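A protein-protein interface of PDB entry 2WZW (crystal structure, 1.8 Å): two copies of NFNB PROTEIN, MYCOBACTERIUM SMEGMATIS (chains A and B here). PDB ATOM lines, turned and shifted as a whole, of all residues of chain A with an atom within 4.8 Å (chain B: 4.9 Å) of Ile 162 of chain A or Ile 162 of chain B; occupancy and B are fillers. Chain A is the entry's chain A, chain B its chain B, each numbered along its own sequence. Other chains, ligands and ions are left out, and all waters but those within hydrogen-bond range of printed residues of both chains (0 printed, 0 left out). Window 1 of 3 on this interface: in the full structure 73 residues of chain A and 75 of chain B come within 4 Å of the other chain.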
ATOM      1  N   ALA A  52     -20.248  36.861  22.443  1.00  0.00           N
ATOM      2  CA  ALA A  52     -20.855  35.677  23.037  1.00  0.00           C
ATOM      3  C   ALA A  52     -21.510  36.072  24.404  1.00  0.00           C
ATOM      4  O   ALA A  52     -20.919  36.856  25.177  1.00  0.00           O
ATOM      5  CB  ALA A  52     -19.777  34.611  23.285  1.00  0.00           C
ATOM      6  N   PRO A  53     -22.701  35.523  24.724  1.00  0.00           N
ATOM      7  CA  PRO A  53     -23.284  35.769  26.049  1.00  0.00           C
ATOM      8  C   PRO A  53     -22.594  34.881  27.102  1.00  0.00           C
ATOM      9  O   PRO A  53     -21.840  33.951  26.766  1.00  0.00           O
ATOM     10  CB  PRO A  53     -24.751  35.355  25.873  1.00  0.00           C
ATOM     11  CG  PRO A  53     -24.688  34.227  24.837  1.00  0.00           C
ATOM     12  CD  PRO A  53     -23.546  34.613  23.909  1.00  0.00           C
ATOM     13  N   GLY A 158     -19.387  25.919  30.439  1.00  0.00           N
ATOM     14  CA  GLY A 158     -20.475  26.126  29.483  1.00  0.00           C
ATOM     15  C   GLY A 158     -20.301  27.446  28.739  1.00  0.00           C
ATOM     16  O   GLY A 158     -20.432  27.496  27.508  1.00  0.00           O
ATOM     17  N   ASP A 159     -19.930  28.519  29.472  1.00  0.00           N
ATOM     18  CA  ASP A 159     -19.678  29.842  28.853  1.00  0.00           C
ATOM     19  C   ASP A 159     -18.471  29.807  27.925  1.00  0.00           C
ATOM     20  O   ASP A 159     -18.471  30.474  26.888  1.00  0.00           O
ATOM     21  CB  ASP A 159     -19.521  30.927  29.926  1.00  0.00           C
ATOM     22  CG  ASP A 159     -20.837  31.247  30.629  1.00  0.00           C
ATOM     23  OD1 ASP A 159     -21.912  30.815  30.122  1.00  0.00           O
ATOM     24  OD2 ASP A 159     -20.799  31.913  31.676  1.00  0.00           O
ATOM     25  N   MET A 160     -17.444  29.012  28.277  1.00  0.00           N
ATOM     26  CA  MET A 160     -16.256  28.844  27.414  1.00  0.00           C
ATOM     27  C   MET A 160     -16.696  28.224  26.066  1.00  0.00           C
ATOM     28  O   MET A 160     -16.199  28.632  25.013  1.00  0.00           O
ATOM     29  CB  MET A 160     -15.187  27.967  28.085  1.00  0.00           C
ATOM     30  CG  MET A 160     -14.642  28.538  29.401  1.00  0.00           C
ATOM     31  SD  MET A 160     -13.703  30.271  29.168  1.00  0.00           S
ATOM     32  CE  MET A 160     -12.387  29.727  27.784  1.00  0.00           C
ATOM     33  N   GLY A 161     -17.621  27.248  26.116  1.00  0.00           N
ATOM     34  CA  GLY A 161     -18.167  26.585  24.938  1.00  0.00           C
ATOM     35  C   GLY A 161     -18.967  27.556  24.084  1.00  0.00           C
ATOM     36  O   GLY A 161     -18.846  27.549  22.858  1.00  0.00           O
ATOM     37  N   ILE A 162     -19.797  28.406  24.724  1.00  0.00           N
ATOM     38  CA  ILE A 162     -20.553  29.459  24.012  1.00  0.00           C
ATOM     39  C   ILE A 162     -19.553  30.311  23.220  1.00  0.00           C
ATOM     40  O   ILE A 162     -19.758  30.542  22.028  1.00  0.00           O
ATOM     41  CB  ILE A 162     -21.401  30.329  24.980  1.00  0.00           C
ATOM     42  CG1 ILE A 162     -22.550  29.476  25.585  1.00  0.00           C
ATOM     43  CG2 ILE A 162     -21.969  31.603  24.246  1.00  0.00           C
ATOM     44  CD1 ILE A 162     -23.390  30.228  26.637  1.00  0.00           C
ATOM     45  N   TYR A 163     -18.480  30.770  23.890  1.00  0.00           N
ATOM     46  CA  TYR A 163     -17.440  31.564  23.222  1.00  0.00           C
ATOM     47  C   TYR A 163     -16.789  30.803  22.051  1.00  0.00           C
ATOM     48  O   TYR A 163     -16.658  31.361  20.959  1.00  0.00           O
ATOM     49  CB  TYR A 163     -16.365  32.030  24.229  1.00  0.00           C
ATOM     50  CG  TYR A 163     -15.217  32.723  23.530  1.00  0.00           C
ATOM     51  CD1 TYR A 163     -15.280  34.081  23.225  1.00  0.00           C
ATOM     52  CD2 TYR A 163     -14.090  32.008  23.119  1.00  0.00           C
ATOM     53  CE1 TYR A 163     -14.259  34.706  22.510  1.00  0.00           C
ATOM     54  CE2 TYR A 163     -13.079  32.616  22.378  1.00  0.00           C
ATOM     55  CZ  TYR A 163     -13.168  33.964  22.079  1.00  0.00           C
ATOM     56  OH  TYR A 163     -12.152  34.569  21.385  1.00  0.00           O
ATOM     57  N   ALA A 164     -16.342  29.544  22.292  1.00  0.00           N
ATOM     58  CA  ALA A 164     -15.665  28.725  21.272  1.00  0.00           C
ATOM     59  C   ALA A 164     -16.504  28.615  19.982  1.00  0.00           C
ATOM     60  O   ALA A 164     -15.981  28.803  18.891  1.00  0.00           O
ATOM     61  CB  ALA A 164     -15.385  27.322  21.838  1.00  0.00           C
ATOM     62  N   GLN A 165     -17.801  28.349  20.110  1.00  0.00           N
ATOM     63  CA  GLN A 165     -18.679  28.222  18.943  1.00  0.00           C
ATOM     64  C   GLN A 165     -18.886  29.573  18.273  1.00  0.00           C
ATOM     65  O   GLN A 165     -18.887  29.633  17.046  1.00  0.00           O
ATOM     66  CB  GLN A 165     -20.013  27.550  19.290  1.00  0.00           C
ATOM     67  CG  GLN A 165     -20.964  27.364  18.080  1.00  0.00           C
ATOM     68  CD  GLN A 165     -20.524  26.356  17.025  1.00  0.00           C
ATOM     69  OE1 GLN A 165     -19.331  26.070  16.837  1.00  0.00           O
ATOM     70  NE2 GLN A 165     -21.491  25.833  16.260  1.00  0.00           N
ATOM     71  N   THR A 166     -19.021  30.663  19.058  1.00  0.00           N
ATOM     72  CA  THR A 166     -19.137  32.008  18.469  1.00  0.00           C
ATOM     73  C   THR A 166     -17.905  32.286  17.624  1.00  0.00           C
ATOM     74  O   THR A 166     -18.035  32.771  16.506  1.00  0.00           O
ATOM     75  CB  THR A 166     -19.308  33.108  19.524  1.00  0.00           C
ATOM     76  OG1 THR A 166     -20.340  32.720  20.425  1.00  0.00           O
ATOM     77  CG2 THR A 166     -19.707  34.468  18.887  1.00  0.00           C
ATOM     78  N   MET A 168     -15.701  30.056  16.244  1.00  0.00           N
ATOM     79  CA  MET A 168     -15.618  29.191  15.061  1.00  0.00           C
ATOM     80  C   MET A 168     -16.570  29.632  13.951  1.00  0.00           C
ATOM     81  O   MET A 168     -16.210  29.543  12.771  1.00  0.00           O
ATOM     82  CB  MET A 168     -15.808  27.707  15.423  1.00  0.00           C
ATOM     83  CG  MET A 168     -14.621  27.159  16.236  1.00  0.00           C
ATOM     84  SD  MET A 168     -14.778  25.233  16.586  1.00  0.00           S
ATOM     85  CE  MET A 168     -16.151  25.242  18.024  1.00  0.00           C
ATOM     86  N   ALA B  52     -24.092  21.490  15.846  1.00  0.00           N
ATOM     87  CA  ALA B  52     -23.025  21.937  16.745  1.00  0.00           C
ATOM     88  C   ALA B  52     -21.927  20.821  16.853  1.00  0.00           C
ATOM     89  O   ALA B  52     -22.268  19.635  16.915  1.00  0.00           O
ATOM     90  CB  ALA B  52     -23.598  22.184  18.135  1.00  0.00           C
ATOM     91  N   PRO B  53     -20.627  21.186  16.920  1.00  0.00           N
ATOM     92  CA  PRO B  53     -19.585  20.169  17.151  1.00  0.00           C
ATOM     93  C   PRO B  53     -19.538  19.800  18.644  1.00  0.00           C
ATOM     94  O   PRO B  53     -20.177  20.459  19.475  1.00  0.00           O
ATOM     95  CB  PRO B  53     -18.295  20.897  16.731  1.00  0.00           C
ATOM     96  CG  PRO B  53     -18.565  22.352  17.132  1.00  0.00           C
ATOM     97  CD  PRO B  53     -20.053  22.549  16.844  1.00  0.00           C
ATOM     98  N   GLY B 158     -18.764  22.249  28.375  1.00  0.00           N
ATOM     99  CA  GLY B 158     -18.296  23.098  27.272  1.00  0.00           C
ATOM    100  C   GLY B 158     -19.104  22.806  26.011  1.00  0.00           C
ATOM    101  O   GLY B 158     -19.590  23.715  25.345  1.00  0.00           O
ATOM    102  N   ASP B 159     -19.295  21.519  25.691  1.00  0.00           N
ATOM    103  CA  ASP B 159     -20.099  21.108  24.528  1.00  0.00           C
ATOM    104  C   ASP B 159     -21.559  21.525  24.651  1.00  0.00           C
ATOM    105  O   ASP B 159     -22.190  21.878  23.644  1.00  0.00           O
ATOM    106  CB  ASP B 159     -19.989  19.589  24.330  1.00  0.00           C
ATOM    107  CG  ASP B 159     -18.605  19.158  23.866  1.00  0.00           C
ATOM    108  OD1 ASP B 159     -17.813  20.036  23.446  1.00  0.00           O
ATOM    109  OD2 ASP B 159     -18.322  17.946  23.901  1.00  0.00           O
ATOM    110  N   MET B 160     -22.108  21.497  25.888  1.00  0.00           N
ATOM    111  CA  MET B 160     -23.491  21.965  26.134  1.00  0.00           C
ATOM    112  C   MET B 160     -23.590  23.467  25.748  1.00  0.00           C
ATOM    113  O   MET B 160     -24.588  23.881  25.139  1.00  0.00           O
ATOM    114  CB  MET B 160     -23.898  21.757  27.615  1.00  0.00           C
ATOM    115  CG  MET B 160     -23.956  20.281  28.037  1.00  0.00           C
ATOM    116  SD  MET B 160     -25.277  19.244  26.977  1.00  0.00           S
ATOM    117  CE  MET B 160     -26.914  20.340  27.390  1.00  0.00           C
ATOM    118  N   GLY B 161     -22.536  24.244  26.050  1.00  0.00           N
ATOM    119  CA  GLY B 161     -22.479  25.673  25.710  1.00  0.00           C
ATOM    120  C   GLY B 161     -22.354  25.887  24.203  1.00  0.00           C
ATOM    121  O   GLY B 161     -22.995  26.781  23.648  1.00  0.00           O
ATOM    122  N   ILE B 162     -21.505  25.073  23.525  1.00  0.00           N
ATOM    123  CA  ILE B 162     -21.382  25.102  22.057  1.00  0.00           C
ATOM    124  C   ILE B 162     -22.791  24.912  21.449  1.00  0.00           C
ATOM    125  O   ILE B 162     -23.215  25.699  20.597  1.00  0.00           O
ATOM    126  CB  ILE B 162     -20.396  24.014  21.566  1.00  0.00           C
ATOM    127  CG1 ILE B 162     -18.946  24.378  21.940  1.00  0.00           C
ATOM    128  CG2 ILE B 162     -20.535  23.776  20.047  1.00  0.00           C
ATOM    129  CD1 ILE B 162     -17.917  23.292  21.505  1.00  0.00           C
ATOM    130  N   TYR B 163     -23.530  23.884  21.915  1.00  0.00           N
ATOM    131  CA  TYR B 163     -24.893  23.661  21.442  1.00  0.00           C
ATOM    132  C   TYR B 163     -25.803  24.872  21.738  1.00  0.00           C
ATOM    133  O   TYR B 163     -26.541  25.296  20.844  1.00  0.00           O
ATOM    134  CB  TYR B 163     -25.498  22.379  22.062  1.00  0.00           C
ATOM    135  CG  TYR B 163     -26.953  22.213  21.689  1.00  0.00           C
ATOM    136  CD1 TYR B 163     -27.321  21.636  20.470  1.00  0.00           C
ATOM    137  CD2 TYR B 163     -27.961  22.718  22.505  1.00  0.00           C
ATOM    138  CE1 TYR B 163     -28.667  21.535  20.095  1.00  0.00           C
ATOM    139  CE2 TYR B 163     -29.305  22.638  22.132  1.00  0.00           C
ATOM    140  CZ  TYR B 163     -29.650  22.054  20.927  1.00  0.00           C
ATOM    141  OH  TYR B 163     -30.980  21.994  20.595  1.00  0.00           O
ATOM    142  N   ALA B 164     -25.816  25.365  23.001  1.00  0.00           N
ATOM    143  CA  ALA B 164     -26.700  26.479  23.404  1.00  0.00           C
ATOM    144  C   ALA B 164     -26.526  27.690  22.479  1.00  0.00           C
ATOM    145  O   ALA B 164     -27.515  28.234  21.989  1.00  0.00           O
ATOM    146  CB  ALA B 164     -26.447  26.869  24.859  1.00  0.00           C
ATOM    147  N   GLN B 165     -25.272  28.065  22.185  1.00  0.00           N
ATOM    148  CA  GLN B 165     -25.008  29.198  21.286  1.00  0.00           C
ATOM    149  C   GLN B 165     -25.433  28.888  19.839  1.00  0.00           C
ATOM    150  O   GLN B 165     -25.997  29.769  19.187  1.00  0.00           O
ATOM    151  CB  GLN B 165     -23.531  29.688  21.363  1.00  0.00           C
ATOM    152  CG  GLN B 165     -23.223  30.939  20.486  1.00  0.00           C
ATOM    153  CD  GLN B 165     -23.894  32.249  20.895  1.00  0.00           C
ATOM    154  OE1 GLN B 165     -24.995  32.296  21.484  1.00  0.00           O
ATOM    155  NE2 GLN B 165     -23.282  33.370  20.503  1.00  0.00           N
ATOM    156  N   THR B 166     -25.220  27.652  19.358  1.00  0.00           N
ATOM    157  CA  THR B 166     -25.658  27.281  17.997  1.00  0.00           C
ATOM    158  C   THR B 166     -27.185  27.451  17.908  1.00  0.00           C
ATOM    159  O   THR B 166     -27.693  28.058  16.964  1.00  0.00           O
ATOM    160  CB  THR B 166     -25.242  25.827  17.642  1.00  0.00           C
ATOM    161  OG1 THR B 166     -23.837  25.651  17.890  1.00  0.00           O
ATOM    162  CG2 THR B 166     -25.539  25.475  16.193  1.00  0.00           C
ATOM    163  N   MET B 168     -29.236  29.372  19.858  1.00  0.00           N
ATOM    164  CA  MET B 168     -29.622  30.786  19.996  1.00  0.00           C
ATOM    165  C   MET B 168     -29.407  31.569  18.717  1.00  0.00           C
ATOM    166  O   MET B 168     -30.239  32.403  18.370  1.00  0.00           O
ATOM    167  CB  MET B 168     -28.907  31.428  21.218  1.00  0.00           C
ATOM    168  CG  MET B 168     -29.503  30.910  22.542  1.00  0.00           C
ATOM    169  SD  MET B 168     -28.870  31.875  24.091  1.00  0.00           S
ATOM    170  CE  MET B 168     -27.085  31.030  24.327  1.00  0.00           C
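NE2 of Gln 165 of chain A is in hydrogen-bond range of OG1 of Thr 166 of chain B, 2.9 Å away.
The side-chain hydroxyl of Thr 166 of chain A lies within hydrogen-bond range of the side-chain amide nitrogen of Gln 165 of chain B (3.0 Å).
The side-chain hydroxyl (OG1) of Thr 166 of chain A sits at hydrogen-bond distance from the backbone carbonyl oxygen (O) of Ile 162 of chain A.
O of Ile 162 of chain B sits at hydrogen-bond distance from OG1 of Thr 166 of chain B (2.8 Å).
CD of Pro 53 of chain A touches NE2 of Gln 165 of chain B (3.6 Å).
Gly 161 of chain B touches Gly 158 of chain A.
Gly 158 of chain B touches Gly 161 of chain A.
O of Gly 161 of chain A touches CG1 of Ile 162 of chain B, at 3.3 Å.
CG1 of Ile 162 of chain A touches O of Gly 161 of chain B, 3.3 Å away.
Ile 162 of chain A touches Ile 162 of chain B.
Ile 162 of chain A touches Gln 165 of chain B (CG2 to CB, 3.8 Å).
Pro 53 of chain B touches Gln 165 of chain A (CD to OE1, 3.6 Å).
Ile 162 of chain B touches Gln 165 of chain A (O to CG, 3.8 Å).
Met 168 of chain A touches Pro 53 of chain B.
Of the printed residues of chain B, Gly 161 of chain A touches Gly 158, Gly 161 and Ile 162.
Of the printed residues of chain B, Ile 162 of chain A touches Gly 161, Ile 162 and Gln 165.
Printed residues of chain B within 4 Å of Gln 165 of chain A: Pro 53, Ile 162 and Thr 166.
Printed residues of chain B within 4 Å of Met 168 of chain A: Pro 53 (3.9 Å).
Met 160 of chain B touches none of the printed residues of chain A.
Of the printed residues of chain A, Gly 161 of chain B touches Gly 158, Gly 161 and Ile 162.
Of chain A, only Gly 161 (3.3 Å), Ile 162 (3.9 Å) and Gln 165 (3.8 Å) come within 4 Å of Ile 162 of chain B.
The nearest residue of chain A that does not touch Ile 162 of chain B is Met 168 of chain A (4.4 Å).
Along chain A the printed residues that touch a printed residue of chain B span positions 53 to 168.
Among the printed residues, 13 pairs touch across the chains.
Pro 53 of chain A touches Gln 165 of chain B, and with the chains exchanged Gln 165 of chain A touches Pro 53 of chain B.
Gly 161 of chain A touches its own counterpart, Gly 161 of chain B.
Ile 162 of chain A touches Gln 165 of chain B, and with the chains exchanged Gln 165 of chain A touches Ile 162 of chain B.
Met 168 of chain A touches Pro 53 of chain B, but with the chains exchanged Pro 53 of chain A does not touch Met 168 of chain B (4.03 Å).
Of the 13 pairs that touch across the chains among the printed residues, 12 have their exchanged pair printed and touching as well.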
